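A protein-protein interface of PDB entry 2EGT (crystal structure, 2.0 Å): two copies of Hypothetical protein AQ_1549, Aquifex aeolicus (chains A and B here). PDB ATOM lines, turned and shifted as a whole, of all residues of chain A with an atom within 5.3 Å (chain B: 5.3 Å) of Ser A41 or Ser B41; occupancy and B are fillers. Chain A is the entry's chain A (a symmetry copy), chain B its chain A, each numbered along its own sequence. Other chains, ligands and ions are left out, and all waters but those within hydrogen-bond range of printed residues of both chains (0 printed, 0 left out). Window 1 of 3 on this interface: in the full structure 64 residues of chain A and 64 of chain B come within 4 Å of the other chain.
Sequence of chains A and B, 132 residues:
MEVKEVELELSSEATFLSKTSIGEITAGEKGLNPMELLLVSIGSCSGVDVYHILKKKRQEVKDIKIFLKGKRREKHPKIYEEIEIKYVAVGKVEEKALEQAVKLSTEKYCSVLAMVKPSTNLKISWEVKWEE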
ATOM      1  N   PRO A  34      -8.349 -18.728  19.472  1.00  0.00           N
ATOM      2  CA  PRO A  34      -8.063 -19.098  20.859  1.00  0.00           C
ATOM      3  C   PRO A  34      -6.703 -19.755  21.089  1.00  0.00           C
ATOM      4  O   PRO A  34      -6.007 -19.410  22.037  1.00  0.00           O
ATOM      5  CB  PRO A  34      -9.235 -20.008  21.218  1.00  0.00           C
ATOM      6  CG  PRO A  34     -10.364 -19.394  20.429  1.00  0.00           C
ATOM      7  CD  PRO A  34      -9.701 -19.171  19.082  1.00  0.00           C
ATOM      8  N   GLU A  36      -4.063 -19.411  19.252  1.00  0.00           N
ATOM      9  CA  GLU A  36      -3.008 -18.446  18.972  1.00  0.00           C
ATOM     10  C   GLU A  36      -2.906 -17.523  20.188  1.00  0.00           C
ATOM     11  O   GLU A  36      -1.820 -17.077  20.552  1.00  0.00           O
ATOM     12  CB  GLU A  36      -3.314 -17.630  17.708  1.00  0.00           C
ATOM     13  CG  GLU A  36      -3.002 -18.362  16.403  1.00  0.00           C
ATOM     14  CD  GLU A  36      -2.966 -17.430  15.198  1.00  0.00           C
ATOM     15  OE1 GLU A  36      -4.043 -17.065  14.680  1.00  0.00           O
ATOM     16  OE2 GLU A  36      -1.852 -17.051  14.774  1.00  0.00           O
ATOM     17  N   LEU A  37      -4.043 -17.243  20.821  1.00  0.00           N
ATOM     18  CA  LEU A  37      -4.036 -16.394  22.009  1.00  0.00           C
ATOM     19  C   LEU A  37      -3.278 -17.085  23.139  1.00  0.00           C
ATOM     20  O   LEU A  37      -2.668 -16.425  23.980  1.00  0.00           O
ATOM     21  CB  LEU A  37      -5.464 -16.069  22.461  1.00  0.00           C
ATOM     22  CG  LEU A  37      -6.226 -15.072  21.578  1.00  0.00           C
ATOM     23  CD1 LEU A  37      -7.619 -14.828  22.150  1.00  0.00           C
ATOM     24  CD2 LEU A  37      -5.456 -13.761  21.511  1.00  0.00           C
ATOM     25  N   LEU A  38      -3.322 -18.414  23.163  1.00  0.00           N
ATOM     26  CA  LEU A  38      -2.600 -19.162  24.188  1.00  0.00           C
ATOM     27  C   LEU A  38      -1.102 -18.917  23.996  1.00  0.00           C
ATOM     28  O   LEU A  38      -0.376 -18.666  24.962  1.00  0.00           O
ATOM     29  CB  LEU A  38      -2.921 -20.659  24.085  1.00  0.00           C
ATOM     30  CG  LEU A  38      -2.103 -21.601  24.983  1.00  0.00           C
ATOM     31  CD1 LEU A  38      -2.242 -21.188  26.441  1.00  0.00           C
ATOM     32  CD2 LEU A  38      -2.582 -23.044  24.778  1.00  0.00           C
ATOM     33  N   LEU A  39      -0.633 -18.982  22.750  1.00  0.00           N
ATOM     34  CA  LEU A  39       0.783 -18.731  22.484  1.00  0.00           C
ATOM     35  C   LEU A  39       1.120 -17.286  22.878  1.00  0.00           C
ATOM     36  O   LEU A  39       2.185 -17.022  23.432  1.00  0.00           O
ATOM     37  CB  LEU A  39       1.112 -18.980  21.005  1.00  0.00           C
ATOM     38  CG  LEU A  39       0.986 -20.434  20.523  1.00  0.00           C
ATOM     39  CD1 LEU A  39       1.378 -20.505  19.051  1.00  0.00           C
ATOM     40  CD2 LEU A  39       1.888 -21.362  21.352  1.00  0.00           C
ATOM     41  N   VAL A  40       0.213 -16.348  22.604  1.00  0.00           N
ATOM     42  CA  VAL A  40       0.450 -14.958  22.994  1.00  0.00           C
ATOM     43  C   VAL A  40       0.566 -14.879  24.520  1.00  0.00           C
ATOM     44  O   VAL A  40       1.431 -14.176  25.043  1.00  0.00           O
ATOM     45  CB  VAL A  40      -0.693 -14.012  22.532  1.00  0.00           C
ATOM     46  CG1 VAL A  40      -0.560 -12.652  23.216  1.00  0.00           C
ATOM     47  CG2 VAL A  40      -0.634 -13.825  21.017  1.00  0.00           C
ATOM     48  N   SER A  41      -0.309 -15.593  25.228  1.00  0.00           N
ATOM     49  CA  SER A  41      -0.286 -15.604  26.697  1.00  0.00           C
ATOM     50  C   SER A  41       1.054 -16.118  27.197  1.00  0.00           C
ATOM     51  O   SER A  41       1.669 -15.528  28.083  1.00  0.00           O
ATOM     52  CB  SER A  41      -1.388 -16.507  27.260  1.00  0.00           C
ATOM     53  OG  SER A  41      -2.671 -16.054  26.874  1.00  0.00           O
ATOM     54  N   ILE A  42       1.486 -17.244  26.638  1.00  0.00           N
ATOM     55  CA  ILE A  42       2.762 -17.838  27.015  1.00  0.00           C
ATOM     56  C   ILE A  42       3.908 -16.879  26.718  1.00  0.00           C
ATOM     57  O   ILE A  42       4.740 -16.599  27.584  1.00  0.00           O
ATOM     58  CB  ILE A  42       3.022 -19.144  26.234  1.00  0.00           C
ATOM     59  CG1 ILE A  42       2.048 -20.230  26.699  1.00  0.00           C
ATOM     60  CG2 ILE A  42       4.481 -19.581  26.418  1.00  0.00           C
ATOM     61  CD1 ILE A  42       2.054 -21.483  25.830  1.00  0.00           C
ATOM     62  N   GLY A  43       3.943 -16.383  25.484  1.00  0.00           N
ATOM     63  CA  GLY A  43       4.998 -15.479  25.070  1.00  0.00           C
ATOM     64  C   GLY A  43       5.147 -14.197  25.870  1.00  0.00           C
ATOM     65  O   GLY A  43       6.269 -13.808  26.209  1.00  0.00           O
ATOM     66  N   SER A  44       4.033 -13.528  26.163  1.00  0.00           N
ATOM     67  CA  SER A  44       4.083 -12.278  26.919  1.00  0.00           C
ATOM     68  C   SER A  44       4.397 -12.528  28.392  1.00  0.00           C
ATOM     69  O   SER A  44       5.088 -11.740  29.025  1.00  0.00           O
ATOM     70  CB  SER A  44       2.765 -11.503  26.762  1.00  0.00           C
ATOM     71  OG  SER A  44       1.631 -12.311  27.036  1.00  0.00           O
ATOM     72  N   CYS A  45       3.890 -13.634  28.923  1.00  0.00           N
ATOM     73  CA  CYS A  45       4.127 -14.039  30.307  1.00  0.00           C
ATOM     74  C   CYS A  45       5.626 -14.186  30.494  1.00  0.00           C
ATOM     75  O   CYS A  45       6.227 -13.566  31.373  1.00  0.00           O
ATOM     76  CB  CYS A  45       3.464 -15.390  30.540  1.00  0.00           C
ATOM     77  SG  CYS A  45       3.715 -16.338  32.088  1.00  0.00           S
ATOM     78  N   SER A  46       6.218 -15.020  29.646  1.00  0.00           N
ATOM     79  CA  SER A  46       7.645 -15.285  29.702  1.00  0.00           C
ATOM     80  C   SER A  46       8.456 -14.049  29.338  1.00  0.00           C
ATOM     81  O   SER A  46       9.454 -13.737  29.992  1.00  0.00           O
ATOM     82  CB  SER A  46       8.000 -16.437  28.756  1.00  0.00           C
ATOM     83  OG  SER A  46       9.382 -16.732  28.843  1.00  0.00           O
ATOM     84  N   VAL A 112       1.905 -19.062  33.063  1.00  0.00           N
ATOM     85  CA  VAL A 112       1.193 -19.683  31.952  1.00  0.00           C
ATOM     86  C   VAL A 112       1.945 -20.913  31.459  1.00  0.00           C
ATOM     87  O   VAL A 112       1.360 -21.982  31.278  1.00  0.00           O
ATOM     88  CB  VAL A 112       1.006 -18.685  30.782  1.00  0.00           C
ATOM     89  CG1 VAL A 112       0.239 -19.354  29.639  1.00  0.00           C
ATOM     90  CG2 VAL A 112       0.258 -17.449  31.271  1.00  0.00           C
ATOM     91  N   PRO B  34      -1.149 -11.156  30.741  1.00  0.00           N
ATOM     92  CA  PRO B  34      -0.964 -12.507  30.210  1.00  0.00           C
ATOM     93  C   PRO B  34      -1.851 -13.580  30.839  1.00  0.00           C
ATOM     94  O   PRO B  34      -2.416 -14.404  30.130  1.00  0.00           O
ATOM     95  CB  PRO B  34       0.526 -12.758  30.428  1.00  0.00           C
ATOM     96  CG  PRO B  34       1.111 -11.384  30.228  1.00  0.00           C
ATOM     97  CD  PRO B  34       0.154 -10.530  31.040  1.00  0.00           C
ATOM     98  N   GLU B  36      -4.712 -13.115  32.275  1.00  0.00           N
ATOM     99  CA  GLU B  36      -6.105 -12.845  31.940  1.00  0.00           C
ATOM    100  C   GLU B  36      -6.327 -13.329  30.506  1.00  0.00           C
ATOM    101  O   GLU B  36      -7.400 -13.824  30.166  1.00  0.00           O
ATOM    102  CB  GLU B  36      -6.431 -11.349  32.055  1.00  0.00           C
ATOM    103  CG  GLU B  36      -6.673 -10.873  33.487  1.00  0.00           C
ATOM    104  CD  GLU B  36      -7.339  -9.503  33.548  1.00  0.00           C
ATOM    105  OE1 GLU B  36      -6.641  -8.481  33.376  1.00  0.00           O
ATOM    106  OE2 GLU B  36      -8.570  -9.451  33.758  1.00  0.00           O
ATOM    107  N   LEU B  37      -5.305 -13.191  29.665  1.00  0.00           N
ATOM    108  CA  LEU B  37      -5.418 -13.652  28.284  1.00  0.00           C
ATOM    109  C   LEU B  37      -5.571 -15.170  28.253  1.00  0.00           C
ATOM    110  O   LEU B  37      -6.212 -15.716  27.355  1.00  0.00           O
ATOM    111  CB  LEU B  37      -4.192 -13.234  27.463  1.00  0.00           C
ATOM    112  CG  LEU B  37      -4.111 -11.743  27.109  1.00  0.00           C
ATOM    113  CD1 LEU B  37      -2.859 -11.473  26.281  1.00  0.00           C
ATOM    114  CD2 LEU B  37      -5.350 -11.339  26.324  1.00  0.00           C
ATOM    115  N   LEU B  38      -4.978 -15.851  29.228  1.00  0.00           N
ATOM    116  CA  LEU B  38      -5.097 -17.304  29.297  1.00  0.00           C
ATOM    117  C   LEU B  38      -6.566 -17.655  29.542  1.00  0.00           C
ATOM    118  O   LEU B  38      -7.115 -18.553  28.897  1.00  0.00           O
ATOM    119  CB  LEU B  38      -4.214 -17.863  30.422  1.00  0.00           C
ATOM    120  CG  LEU B  38      -4.365 -19.359  30.736  1.00  0.00           C
ATOM    121  CD1 LEU B  38      -4.113 -20.187  29.484  1.00  0.00           C
ATOM    122  CD2 LEU B  38      -3.385 -19.747  31.851  1.00  0.00           C
ATOM    123  N   LEU B  39      -7.212 -16.945  30.467  1.00  0.00           N
ATOM    124  CA  LEU B  39      -8.626 -17.202  30.736  1.00  0.00           C
ATOM    125  C   LEU B  39      -9.442 -16.896  29.472  1.00  0.00           C
ATOM    126  O   LEU B  39     -10.382 -17.619  29.146  1.00  0.00           O
ATOM    127  CB  LEU B  39      -9.119 -16.353  31.917  1.00  0.00           C
ATOM    128  CG  LEU B  39      -8.505 -16.684  33.287  1.00  0.00           C
ATOM    129  CD1 LEU B  39      -9.126 -15.776  34.342  1.00  0.00           C
ATOM    130  CD2 LEU B  39      -8.750 -18.157  33.651  1.00  0.00           C
ATOM    131  N   VAL B  40      -9.083 -15.834  28.751  1.00  0.00           N
ATOM    132  CA  VAL B  40      -9.787 -15.512  27.510  1.00  0.00           C
ATOM    133  C   VAL B  40      -9.609 -16.668  26.519  1.00  0.00           C
ATOM    134  O   VAL B  40     -10.560 -17.059  25.841  1.00  0.00           O
ATOM    135  CB  VAL B  40      -9.261 -14.207  26.853  1.00  0.00           C
ATOM    136  CG1 VAL B  40      -9.800 -14.079  25.429  1.00  0.00           C
ATOM    137  CG2 VAL B  40      -9.702 -12.996  27.672  1.00  0.00           C
ATOM    138  N   SER B  41      -8.391 -17.205  26.433  1.00  0.00           N
ATOM    139  CA  SER B  41      -8.106 -18.324  25.526  1.00  0.00           C
ATOM    140  C   SER B  41      -8.978 -19.518  25.876  1.00  0.00           C
ATOM    141  O   SER B  41      -9.586 -20.137  25.004  1.00  0.00           O
ATOM    142  CB  SER B  41      -6.639 -18.755  25.627  1.00  0.00           C
ATOM    143  OG  SER B  41      -5.768 -17.702  25.263  1.00  0.00           O
ATOM    144  N   ILE B  42      -9.010 -19.855  27.161  1.00  0.00           N
ATOM    145  CA  ILE B  42      -9.818 -20.971  27.635  1.00  0.00           C
ATOM    146  C   ILE B  42     -11.293 -20.730  27.335  1.00  0.00           C
ATOM    147  O   ILE B  42     -11.968 -21.582  26.753  1.00  0.00           O
ATOM    148  CB  ILE B  42      -9.669 -21.161  29.160  1.00  0.00           C
ATOM    149  CG1 ILE B  42      -8.261 -21.665  29.485  1.00  0.00           C
ATOM    150  CG2 ILE B  42     -10.745 -22.127  29.673  1.00  0.00           C
ATOM    151  CD1 ILE B  42      -7.926 -21.656  30.972  1.00  0.00           C
ATOM    152  N   GLY B  43     -11.783 -19.562  27.742  1.00  0.00           N
ATOM    153  CA  GLY B  43     -13.178 -19.223  27.539  1.00  0.00           C
ATOM    154  C   GLY B  43     -13.676 -19.230  26.104  1.00  0.00           C
ATOM    155  O   GLY B  43     -14.762 -19.749  25.830  1.00  0.00           O
ATOM    156  N   SER B  44     -12.904 -18.646  25.188  1.00  0.00           N
ATOM    157  CA  SER B  44     -13.311 -18.594  23.785  1.00  0.00           C
ATOM    158  C   SER B  44     -13.183 -19.960  23.115  1.00  0.00           C
ATOM    159  O   SER B  44     -13.991 -20.318  22.268  1.00  0.00           O
ATOM    160  CB  SER B  44     -12.495 -17.533  23.029  1.00  0.00           C
ATOM    161  OG  SER B  44     -11.099 -17.684  23.232  1.00  0.00           O
ATOM    162  N   CYS B  45     -12.166 -20.717  23.510  1.00  0.00           N
ATOM    163  CA  CYS B  45     -11.924 -22.064  22.997  1.00  0.00           C
ATOM    164  C   CYS B  45     -13.154 -22.899  23.299  1.00  0.00           C
ATOM    165  O   CYS B  45     -13.763 -23.492  22.406  1.00  0.00           O
ATOM    166  CB  CYS B  45     -10.729 -22.657  23.731  1.00  0.00           C
ATOM    167  SG  CYS B  45     -10.240 -24.412  23.527  1.00  0.00           S
ATOM    168  N   SER B  46     -13.508 -22.935  24.579  1.00  0.00           N
ATOM    169  CA  SER B  46     -14.653 -23.703  25.037  1.00  0.00           C
ATOM    170  C   SER B  46     -15.958 -23.132  24.502  1.00  0.00           C
ATOM    171  O   SER B  46     -16.838 -23.877  24.064  1.00  0.00           O
ATOM    172  CB  SER B  46     -14.685 -23.729  26.568  1.00  0.00           C
ATOM    173  OG  SER B  46     -15.771 -24.519  27.021  1.00  0.00           O
ATOM    174  N   VAL B 112      -7.307 -25.793  24.593  1.00  0.00           N
ATOM    175  CA  VAL B 112      -6.648 -24.981  25.608  1.00  0.00           C
ATOM    176  C   VAL B 112      -6.907 -25.552  26.998  1.00  0.00           C
ATOM    177  O   VAL B 112      -5.984 -25.722  27.795  1.00  0.00           O
ATOM    178  CB  VAL B 112      -7.135 -23.512  25.553  1.00  0.00           C
ATOM    179  CG1 VAL B 112      -6.414 -22.678  26.613  1.00  0.00           C
ATOM    180  CG2 VAL B 112      -6.884 -22.936  24.163  1.00  0.00           C
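OG of Ser B41 sits at hydrogen-bond distance from N of Leu A38 (3.3 Å). The backbone NH (N) of Leu B38 sits at hydrogen-bond distance from the side-chain hydroxyl (OG) of Ser A41 (3.3 Å).
The side-chain sulfur (SG) of Cys A45 is in hydrogen-bond range of the backbone NH (N) of Val A112, at 3.4 Å. The side-chain hydroxyl (OG) of Ser B44 lies within hydrogen-bond range of the backbone carbonyl oxygen (O) of Val B40 (2.7 Å). OG of Ser A41 lies within hydrogen-bond range of O of Leu A37 (2.9 Å). OG of Ser B41 is in hydrogen-bond range of O of Leu B37 (2.9 Å). The backbone carbonyl oxygen (O) of Ser A41 is in hydrogen-bond range of the side-chain hydroxyl (OG) of Ser A44 (3.4 Å). The side-chain sulfur of Cys B45 is in hydrogen-bond range of the backbone NH of Val B112.
Among the printed residues, pairs that only touch across the chains: Leu A37 with Ser B41 (3.3 Å), Ser A41 with Leu B37 (3.3 Å), Ser A44 with Pro B34 (3.4 Å), Pro A34 with Ser B44 (3.4 Å), Pro A34 with Ser B41 (3.7 Å), Ser A41 with Pro B34 (3.7 Å), Leu A38 with Leu B38 (3.7 Å), Pro A34 with Cys B45 (3.8 Å), Cys A45 with Pro B34 (3.8 Å) and Ser A41 with Ser B41 (3.9 Å).
Printed residues of chain B within 4 Å of Leu A38: Leu B38 and Ser B41. Leu A39 touches none of the printed residues of chain B. Ser A41 touches just these residues of chain B: Pro B34, Leu B37, Leu B38 and Ser B41. Ile A42 touches none of the printed residues of chain B. Of the printed residues of chain A, Leu B38 touches Leu A38 and Ser A41. Ser B41 touches just these residues of chain A: Pro A34, Leu A37, Leu A38 and Ser A41. Of the printed residues of chain A, Ser B44 touches Pro A34. Of the printed residues of chain A, Cys B45 touches Pro A34. The nearest printed residue of chain B that does not touch Ser A41 is Glu B36 (5.8 Å). The nearest printed residue of chain A that does not touch Ser B41 is Glu A36 (5.8 Å).
Hydrophobic or aromatic side chains of chain B that line the printed part of chain A: Pro B34, Leu B37 and Leu B38. Along chain B the printed residues that touch a printed residue of chain A span positions 34 to 45. Of the 13 printed residues of chain A, 6 touch a printed residue of chain B. Hydrophobic or aromatic side chains of chain A that line the printed part of chain B: Pro A34, Leu A37 and Leu A38.
Pro A34 touches Cys B45, and with the chains exchanged Cys A45 touches Pro B34. Leu A38 touches its own counterpart, Leu B38. Leu A38 touches Ser B41, and with the chains exchanged Ser A41 touches Leu B38. Ser A41 touches its own counterpart, Ser B41. Of the 12 pairs that touch across the chains among the printed residues, 12 have their exchanged pair printed and touching as well.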
